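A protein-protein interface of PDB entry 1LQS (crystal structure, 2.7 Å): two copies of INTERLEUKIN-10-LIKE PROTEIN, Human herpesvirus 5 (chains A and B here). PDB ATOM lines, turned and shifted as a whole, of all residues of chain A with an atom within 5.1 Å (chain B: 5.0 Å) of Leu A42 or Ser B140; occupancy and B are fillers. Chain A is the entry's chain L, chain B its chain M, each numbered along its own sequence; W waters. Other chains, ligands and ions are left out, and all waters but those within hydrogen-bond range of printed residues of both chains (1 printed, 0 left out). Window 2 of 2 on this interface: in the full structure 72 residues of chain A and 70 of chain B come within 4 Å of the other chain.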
ATOM      1  N   PHE A  35      29.187 -17.872  22.691  1.00  0.00           N
ATOM      2  CA  PHE A  35      27.865 -17.877  22.103  1.00  0.00           C
ATOM      3  C   PHE A  35      26.905 -16.927  22.779  1.00  0.00           C
ATOM      4  O   PHE A  35      26.069 -16.316  22.126  1.00  0.00           O
ATOM      5  CB  PHE A  35      27.249 -19.274  22.145  1.00  0.00           C
ATOM      6  CG  PHE A  35      25.910 -19.349  21.471  1.00  0.00           C
ATOM      7  CD1 PHE A  35      25.818 -19.264  20.078  1.00  0.00           C
ATOM      8  CD2 PHE A  35      24.743 -19.445  22.224  1.00  0.00           C
ATOM      9  CE1 PHE A  35      24.596 -19.268  19.443  1.00  0.00           C
ATOM     10  CE2 PHE A  35      23.501 -19.449  21.603  1.00  0.00           C
ATOM     11  CZ  PHE A  35      23.425 -19.360  20.201  1.00  0.00           C
ATOM     12  N   VAL A  38      26.907 -13.179  21.480  1.00  0.00           N
ATOM     13  CA  VAL A  38      26.360 -12.907  20.169  1.00  0.00           C
ATOM     14  C   VAL A  38      24.988 -13.539  19.963  1.00  0.00           C
ATOM     15  O   VAL A  38      24.404 -13.456  18.877  1.00  0.00           O
ATOM     16  CB  VAL A  38      27.361 -13.421  19.102  1.00  0.00           C
ATOM     17  CG1 VAL A  38      27.634 -14.912  19.308  1.00  0.00           C
ATOM     18  CG2 VAL A  38      26.819 -13.184  17.708  1.00  0.00           C
ATOM     19  N   LYS A  39      24.468 -14.151  21.021  1.00  0.00           N
ATOM     20  CA  LYS A  39      23.179 -14.842  20.974  1.00  0.00           C
ATOM     21  C   LYS A  39      22.035 -13.979  20.441  1.00  0.00           C
ATOM     22  O   LYS A  39      21.268 -14.410  19.575  1.00  0.00           O
ATOM     23  CB  LYS A  39      22.847 -15.371  22.370  1.00  0.00           C
ATOM     24  CG  LYS A  39      21.782 -16.442  22.428  1.00  0.00           C
ATOM     25  CD  LYS A  39      21.578 -16.881  23.873  1.00  0.00           C
ATOM     26  CE  LYS A  39      20.532 -17.956  23.989  1.00  0.00           C
ATOM     27  NZ  LYS A  39      19.988 -17.982  25.355  1.00  0.00           N
ATOM     28  N   PRO A  40      21.889 -12.750  20.959  1.00  0.00           N
ATOM     29  CA  PRO A  40      20.796 -11.914  20.451  1.00  0.00           C
ATOM     30  C   PRO A  40      20.864 -11.587  18.952  1.00  0.00           C
ATOM     31  O   PRO A  40      19.832 -11.409  18.313  1.00  0.00           O
ATOM     32  CB  PRO A  40      20.836 -10.675  21.364  1.00  0.00           C
ATOM     33  CG  PRO A  40      22.199 -10.702  21.969  1.00  0.00           C
ATOM     34  CD  PRO A  40      22.476 -12.162  22.174  1.00  0.00           C
ATOM     35  N   THR A  41      22.064 -11.513  18.386  1.00  0.00           N
ATOM     36  CA  THR A  41      22.175 -11.255  16.955  1.00  0.00           C
ATOM     37  C   THR A  41      21.741 -12.505  16.177  1.00  0.00           C
ATOM     38  O   THR A  41      20.788 -12.459  15.390  1.00  0.00           O
ATOM     39  CB  THR A  41      23.614 -10.911  16.542  1.00  0.00           C
ATOM     40  OG1 THR A  41      23.987  -9.652  17.109  1.00  0.00           O
ATOM     41  CG2 THR A  41      23.738 -10.837  15.016  1.00  0.00           C
ATOM     42  N   LEU A  42      22.427 -13.622  16.414  1.00  0.00           N
ATOM     43  CA  LEU A  42      22.124 -14.875  15.728  1.00  0.00           C
ATOM     44  C   LEU A  42      20.702 -15.368  15.904  1.00  0.00           C
ATOM     45  O   LEU A  42      20.209 -16.106  15.052  1.00  0.00           O
ATOM     46  CB  LEU A  42      23.081 -15.997  16.163  1.00  0.00           C
ATOM     47  CG  LEU A  42      24.576 -15.785  15.908  1.00  0.00           C
ATOM     48  CD1 LEU A  42      25.341 -17.065  16.176  1.00  0.00           C
ATOM     49  CD2 LEU A  42      24.783 -15.342  14.476  1.00  0.00           C
ATOM     50  N   GLN A  43      20.033 -14.985  16.988  1.00  0.00           N
ATOM     51  CA  GLN A  43      18.666 -15.456  17.190  1.00  0.00           C
ATOM     52  C   GLN A  43      17.596 -14.405  16.907  1.00  0.00           C
ATOM     53  O   GLN A  43      16.487 -14.481  17.447  1.00  0.00           O
ATOM     54  CB  GLN A  43      18.482 -16.006  18.611  1.00  0.00           C
ATOM     55  CG  GLN A  43      19.390 -17.188  18.976  1.00  0.00           C
ATOM     56  CD  GLN A  43      19.043 -17.804  20.325  1.00  0.00           C
ATOM     57  OE1 GLN A  43      18.705 -17.102  21.269  1.00  0.00           O
ATOM     58  NE2 GLN A  43      19.137 -19.122  20.419  1.00  0.00           N
ATOM     59  N   ARG A  44      17.914 -13.436  16.049  1.00  0.00           N
ATOM     60  CA  ARG A  44      16.945 -12.393  15.716  1.00  0.00           C
ATOM     61  C   ARG A  44      15.872 -12.870  14.744  1.00  0.00           C
ATOM     62  O   ARG A  44      14.705 -12.981  15.123  1.00  0.00           O
ATOM     63  CB  ARG A  44      17.639 -11.133  15.174  1.00  0.00           C
ATOM     64  CG  ARG A  44      17.635 -10.009  16.214  1.00  0.00           C
ATOM     65  CD  ARG A  44      17.855  -8.610  15.653  1.00  0.00           C
ATOM     66  NE  ARG A  44      19.179  -8.432  15.066  1.00  0.00           N
ATOM     67  CZ  ARG A  44      19.807  -7.262  14.997  1.00  0.00           C
ATOM     68  NH1 ARG A  44      19.222  -6.172  15.489  1.00  0.00           N
ATOM     69  NH2 ARG A  44      21.006  -7.173  14.430  1.00  0.00           N
ATOM     70  N   ASP A  46      15.211 -15.845  13.417  1.00  0.00           N
ATOM     71  CA  ASP A  46      14.637 -17.012  14.064  1.00  0.00           C
ATOM     72  C   ASP A  46      13.155 -17.275  13.815  1.00  0.00           C
ATOM     73  O   ASP A  46      12.302 -16.635  14.444  1.00  0.00           O
ATOM     74  CB  ASP A  46      14.830 -16.938  15.590  1.00  0.00           C
ATOM     75  CG  ASP A  46      16.069 -17.677  16.076  1.00  0.00           C
ATOM     76  OD1 ASP A  46      16.064 -18.141  17.245  1.00  0.00           O
ATOM     77  OD2 ASP A  46      17.048 -17.785  15.302  1.00  0.00           O
ATOM     78  N   TYR A  85      27.143 -12.879   8.621  1.00  0.00           N
ATOM     79  CA  TYR A  85      27.361 -12.040   9.797  1.00  0.00           C
ATOM     80  C   TYR A  85      28.784 -11.493   9.834  1.00  0.00           C
ATOM     81  O   TYR A  85      29.584 -11.863  10.692  1.00  0.00           O
ATOM     82  CB  TYR A  85      27.096 -12.838  11.065  1.00  0.00           C
ATOM     83  CG  TYR A  85      25.696 -13.378  11.170  1.00  0.00           C
ATOM     84  CD1 TYR A  85      25.424 -14.727  10.949  1.00  0.00           C
ATOM     85  CD2 TYR A  85      24.651 -12.556  11.551  1.00  0.00           C
ATOM     86  CE1 TYR A  85      24.151 -15.239  11.120  1.00  0.00           C
ATOM     87  CE2 TYR A  85      23.370 -13.056  11.724  1.00  0.00           C
ATOM     88  CZ  TYR A  85      23.123 -14.392  11.513  1.00  0.00           C
ATOM     89  OH  TYR A  85      21.850 -14.873  11.733  1.00  0.00           O
ATOM     90  N   LEU A  88      30.324 -10.536  13.395  1.00  0.00           N
ATOM     91  CA  LEU A  88      30.694 -11.571  14.347  1.00  0.00           C
ATOM     92  C   LEU A  88      31.795 -12.495  13.858  1.00  0.00           C
ATOM     93  O   LEU A  88      32.036 -13.528  14.471  1.00  0.00           O
ATOM     94  CB  LEU A  88      29.480 -12.427  14.673  1.00  0.00           C
ATOM     95  CG  LEU A  88      28.124 -11.736  14.618  1.00  0.00           C
ATOM     96  CD1 LEU A  88      27.040 -12.799  14.570  1.00  0.00           C
ATOM     97  CD2 LEU A  88      27.953 -10.808  15.811  1.00  0.00           C
ATOM     98  N   LEU A  92      32.682 -15.975  15.576  1.00  0.00           N
ATOM     99  CA  LEU A  92      32.453 -17.158  14.764  1.00  0.00           C
ATOM    100  C   LEU A  92      33.696 -18.031  14.681  1.00  0.00           C
ATOM    101  O   LEU A  92      33.623 -19.228  14.926  1.00  0.00           O
ATOM    102  CB  LEU A  92      31.988 -16.753  13.365  1.00  0.00           C
ATOM    103  CG  LEU A  92      30.532 -16.276  13.318  1.00  0.00           C
ATOM    104  CD1 LEU A  92      30.207 -15.699  11.959  1.00  0.00           C
ATOM    105  CD2 LEU A  92      29.605 -17.436  13.640  1.00  0.00           C
ATOM    106  N   MET A  95      34.609 -19.888  17.947  1.00  0.00           N
ATOM    107  CA  MET A  95      33.780 -21.049  18.169  1.00  0.00           C
ATOM    108  C   MET A  95      34.179 -22.198  17.252  1.00  0.00           C
ATOM    109  O   MET A  95      34.349 -23.327  17.724  1.00  0.00           O
ATOM    110  CB  MET A  95      32.288 -20.695  17.988  1.00  0.00           C
ATOM    111  CG  MET A  95      31.712 -19.809  19.117  1.00  0.00           C
ATOM    112  SD  MET A  95      29.905 -19.490  19.119  1.00  0.00           S
ATOM    113  CE  MET A  95      29.752 -18.423  17.670  1.00  0.00           C
ATOM    114  N   ARG B 136      21.571 -19.623   8.576  1.00  0.00           N
ATOM    115  CA  ARG B 136      20.920 -18.880   9.639  1.00  0.00           C
ATOM    116  C   ARG B 136      20.404 -19.840  10.715  1.00  0.00           C
ATOM    117  O   ARG B 136      20.831 -19.770  11.869  1.00  0.00           O
ATOM    118  CB  ARG B 136      19.772 -18.053   9.057  1.00  0.00           C
ATOM    119  CG  ARG B 136      19.842 -16.580   9.384  1.00  0.00           C
ATOM    120  CD  ARG B 136      19.478 -15.707   8.174  1.00  0.00           C
ATOM    121  NE  ARG B 136      20.568 -15.622   7.199  1.00  0.00           N
ATOM    122  CZ  ARG B 136      20.593 -14.781   6.167  1.00  0.00           C
ATOM    123  NH1 ARG B 136      19.585 -13.947   5.961  1.00  0.00           N
ATOM    124  NH2 ARG B 136      21.633 -14.763   5.348  1.00  0.00           N
ATOM    125  N   LYS B 137      19.495 -20.738  10.347  1.00  0.00           N
ATOM    126  CA  LYS B 137      18.964 -21.691  11.322  1.00  0.00           C
ATOM    127  C   LYS B 137      20.098 -22.429  12.034  1.00  0.00           C
ATOM    128  O   LYS B 137      19.997 -22.774  13.210  1.00  0.00           O
ATOM    129  CB  LYS B 137      18.067 -22.725  10.644  1.00  0.00           C
ATOM    130  CG  LYS B 137      16.615 -22.674  11.093  1.00  0.00           C
ATOM    131  CD  LYS B 137      16.475 -22.611  12.616  1.00  0.00           C
ATOM    132  CE  LYS B 137      15.047 -22.234  13.016  1.00  0.00           C
ATOM    133  NZ  LYS B 137      14.975 -21.653  14.389  1.00  0.00           N
ATOM    134  N   GLY B 138      21.180 -22.655  11.300  1.00  0.00           N
ATOM    135  CA  GLY B 138      22.316 -23.368  11.841  1.00  0.00           C
ATOM    136  C   GLY B 138      23.039 -22.688  12.981  1.00  0.00           C
ATOM    137  O   GLY B 138      23.296 -23.313  14.007  1.00  0.00           O
ATOM    138  N   LEU B 139      23.385 -21.419  12.806  1.00  0.00           N
ATOM    139  CA  LEU B 139      24.090 -20.695  13.846  1.00  0.00           C
ATOM    140  C   LEU B 139      23.195 -20.331  15.045  1.00  0.00           C
ATOM    141  O   LEU B 139      23.677 -20.156  16.159  1.00  0.00           O
ATOM    142  CB  LEU B 139      24.706 -19.424  13.269  1.00  0.00           C
ATOM    143  CG  LEU B 139      25.910 -19.463  12.328  1.00  0.00           C
ATOM    144  CD1 LEU B 139      26.948 -20.422  12.864  1.00  0.00           C
ATOM    145  CD2 LEU B 139      25.475 -19.860  10.964  1.00  0.00           C
ATOM    146  N   SER B 140      21.892 -20.231  14.823  1.00  0.00           N
ATOM    147  CA  SER B 140      21.001 -19.856  15.903  1.00  0.00           C
ATOM    148  C   SER B 140      20.730 -21.029  16.803  1.00  0.00           C
ATOM    149  O   SER B 140      20.206 -20.863  17.902  1.00  0.00           O
ATOM    150  CB  SER B 140      19.681 -19.328  15.353  1.00  0.00           C
ATOM    151  OG  SER B 140      18.962 -20.363  14.710  1.00  0.00           O
ATOM    152  N   GLU B 141      21.068 -22.224  16.327  1.00  0.00           N
ATOM    153  CA  GLU B 141      20.855 -23.431  17.109  1.00  0.00           C
ATOM    154  C   GLU B 141      22.153 -23.938  17.750  1.00  0.00           C
ATOM    155  O   GLU B 141      22.180 -25.018  18.339  1.00  0.00           O
ATOM    156  CB  GLU B 141      20.219 -24.516  16.236  1.00  0.00           C
ATOM    157  CG  GLU B 141      18.790 -24.203  15.826  1.00  0.00           C
ATOM    158  CD  GLU B 141      17.879 -25.426  15.889  1.00  0.00           C
ATOM    159  OE1 GLU B 141      18.119 -26.391  15.140  1.00  0.00           O
ATOM    160  OE2 GLU B 141      16.922 -25.431  16.695  1.00  0.00           O
ATOM    161  N   LEU B 142      23.220 -23.149  17.637  1.00  0.00           N
ATOM    162  CA  LEU B 142      24.506 -23.505  18.226  1.00  0.00           C
ATOM    163  C   LEU B 142      24.352 -23.923  19.693  1.00  0.00           C
ATOM    164  O   LEU B 142      24.955 -24.898  20.136  1.00  0.00           O
ATOM    165  CB  LEU B 142      25.482 -22.333  18.115  1.00  0.00           C
ATOM    166  CG  LEU B 142      26.151 -22.228  16.747  1.00  0.00           C
ATOM    167  CD1 LEU B 142      27.084 -21.021  16.681  1.00  0.00           C
ATOM    168  CD2 LEU B 142      26.929 -23.514  16.496  1.00  0.00           C
ATOM    169  N   ASP B 143      23.549 -23.181  20.445  1.00  0.00           N
ATOM    170  CA  ASP B 143      23.310 -23.531  21.829  1.00  0.00           C
ATOM    171  C   ASP B 143      22.760 -24.967  21.858  1.00  0.00           C
ATOM    172  O   ASP B 143      23.278 -25.819  22.589  1.00  0.00           O
ATOM    173  CB  ASP B 143      22.329 -22.535  22.468  1.00  0.00           C
ATOM    174  CG  ASP B 143      21.056 -22.360  21.650  1.00  0.00           C
ATOM    175  OD1 ASP B 143      21.060 -22.803  20.486  1.00  0.00           O
ATOM    176  OD2 ASP B 143      20.062 -21.782  22.159  1.00  0.00           O
HETATM  177  O   HOH W   1      16.524 -19.233  12.785  1.00  0.00           O
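NE2 of Gln A43 is in hydrogen-bond range of OD2 of Asp B143. NE2 of Gln A43 lies within hydrogen-bond range of O of Ser B140 (3.2 Å). OD2 of Asp A46 lies close to OG of Ser B140.
The side-chain hydroxyl (OG) of Ser B140 lies within hydrogen-bond range of the backbone carbonyl oxygen (O) of Lys B137 (3.0 Å). O of Arg B136 is in hydrogen-bond range of OG of Ser B140.
CE1 of Phe A35 touches O of Leu B139, 3.5 Å away. CE1 of Phe A35 touches CB of Leu B142 (3.5 Å). Phe A35 touches Asp B143 (CE2 to CB, 3.4 Å). O of Leu B139 touches CD1 of Leu A42, at 3.5 Å. Leu A42 touches Ser B140. OH of Tyr A85 touches CG of Arg B136, at 3.5 Å. CE of Met A95 touches CD1 of Leu B142, 3.9 Å away.
Leu A42 touches two residues of chain B. Ser B140 touches just these residues of chain A: Leu A42 (3.3 Å), Gln A43 (3.2 Å) and Asp A46 (3.1 Å). Of the printed residues of chain A, Asp B143 touches Phe A35 and Gln A43. Of the printed residues of chain B, Gln A43 touches Ser B140 and Asp B143. Of the printed residues of chain B, Met A95 touches Leu B142 (3.9 Å). The nearest printed residue of chain B that does not touch Met A95 is Leu B139 (5.9 Å).
Hydrophobic or aromatic side chains of chain B that line the printed part of chain A: Leu B139 and Leu B142.
No position is printed for both chains. Of the 10 pairs that touch across the chains among the printed residues, none has its exchanged pair printed and touching as well.
Water W1 lies within hydrogen-bond range of the side-chain carboxylate (OD2) of Asp A46 (3.0 Å), the side-chain amino group (NZ) of Lys B137 (3.3 Å) and the side-chain hydroxyl (OG) of Ser B140 (3.3 Å).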
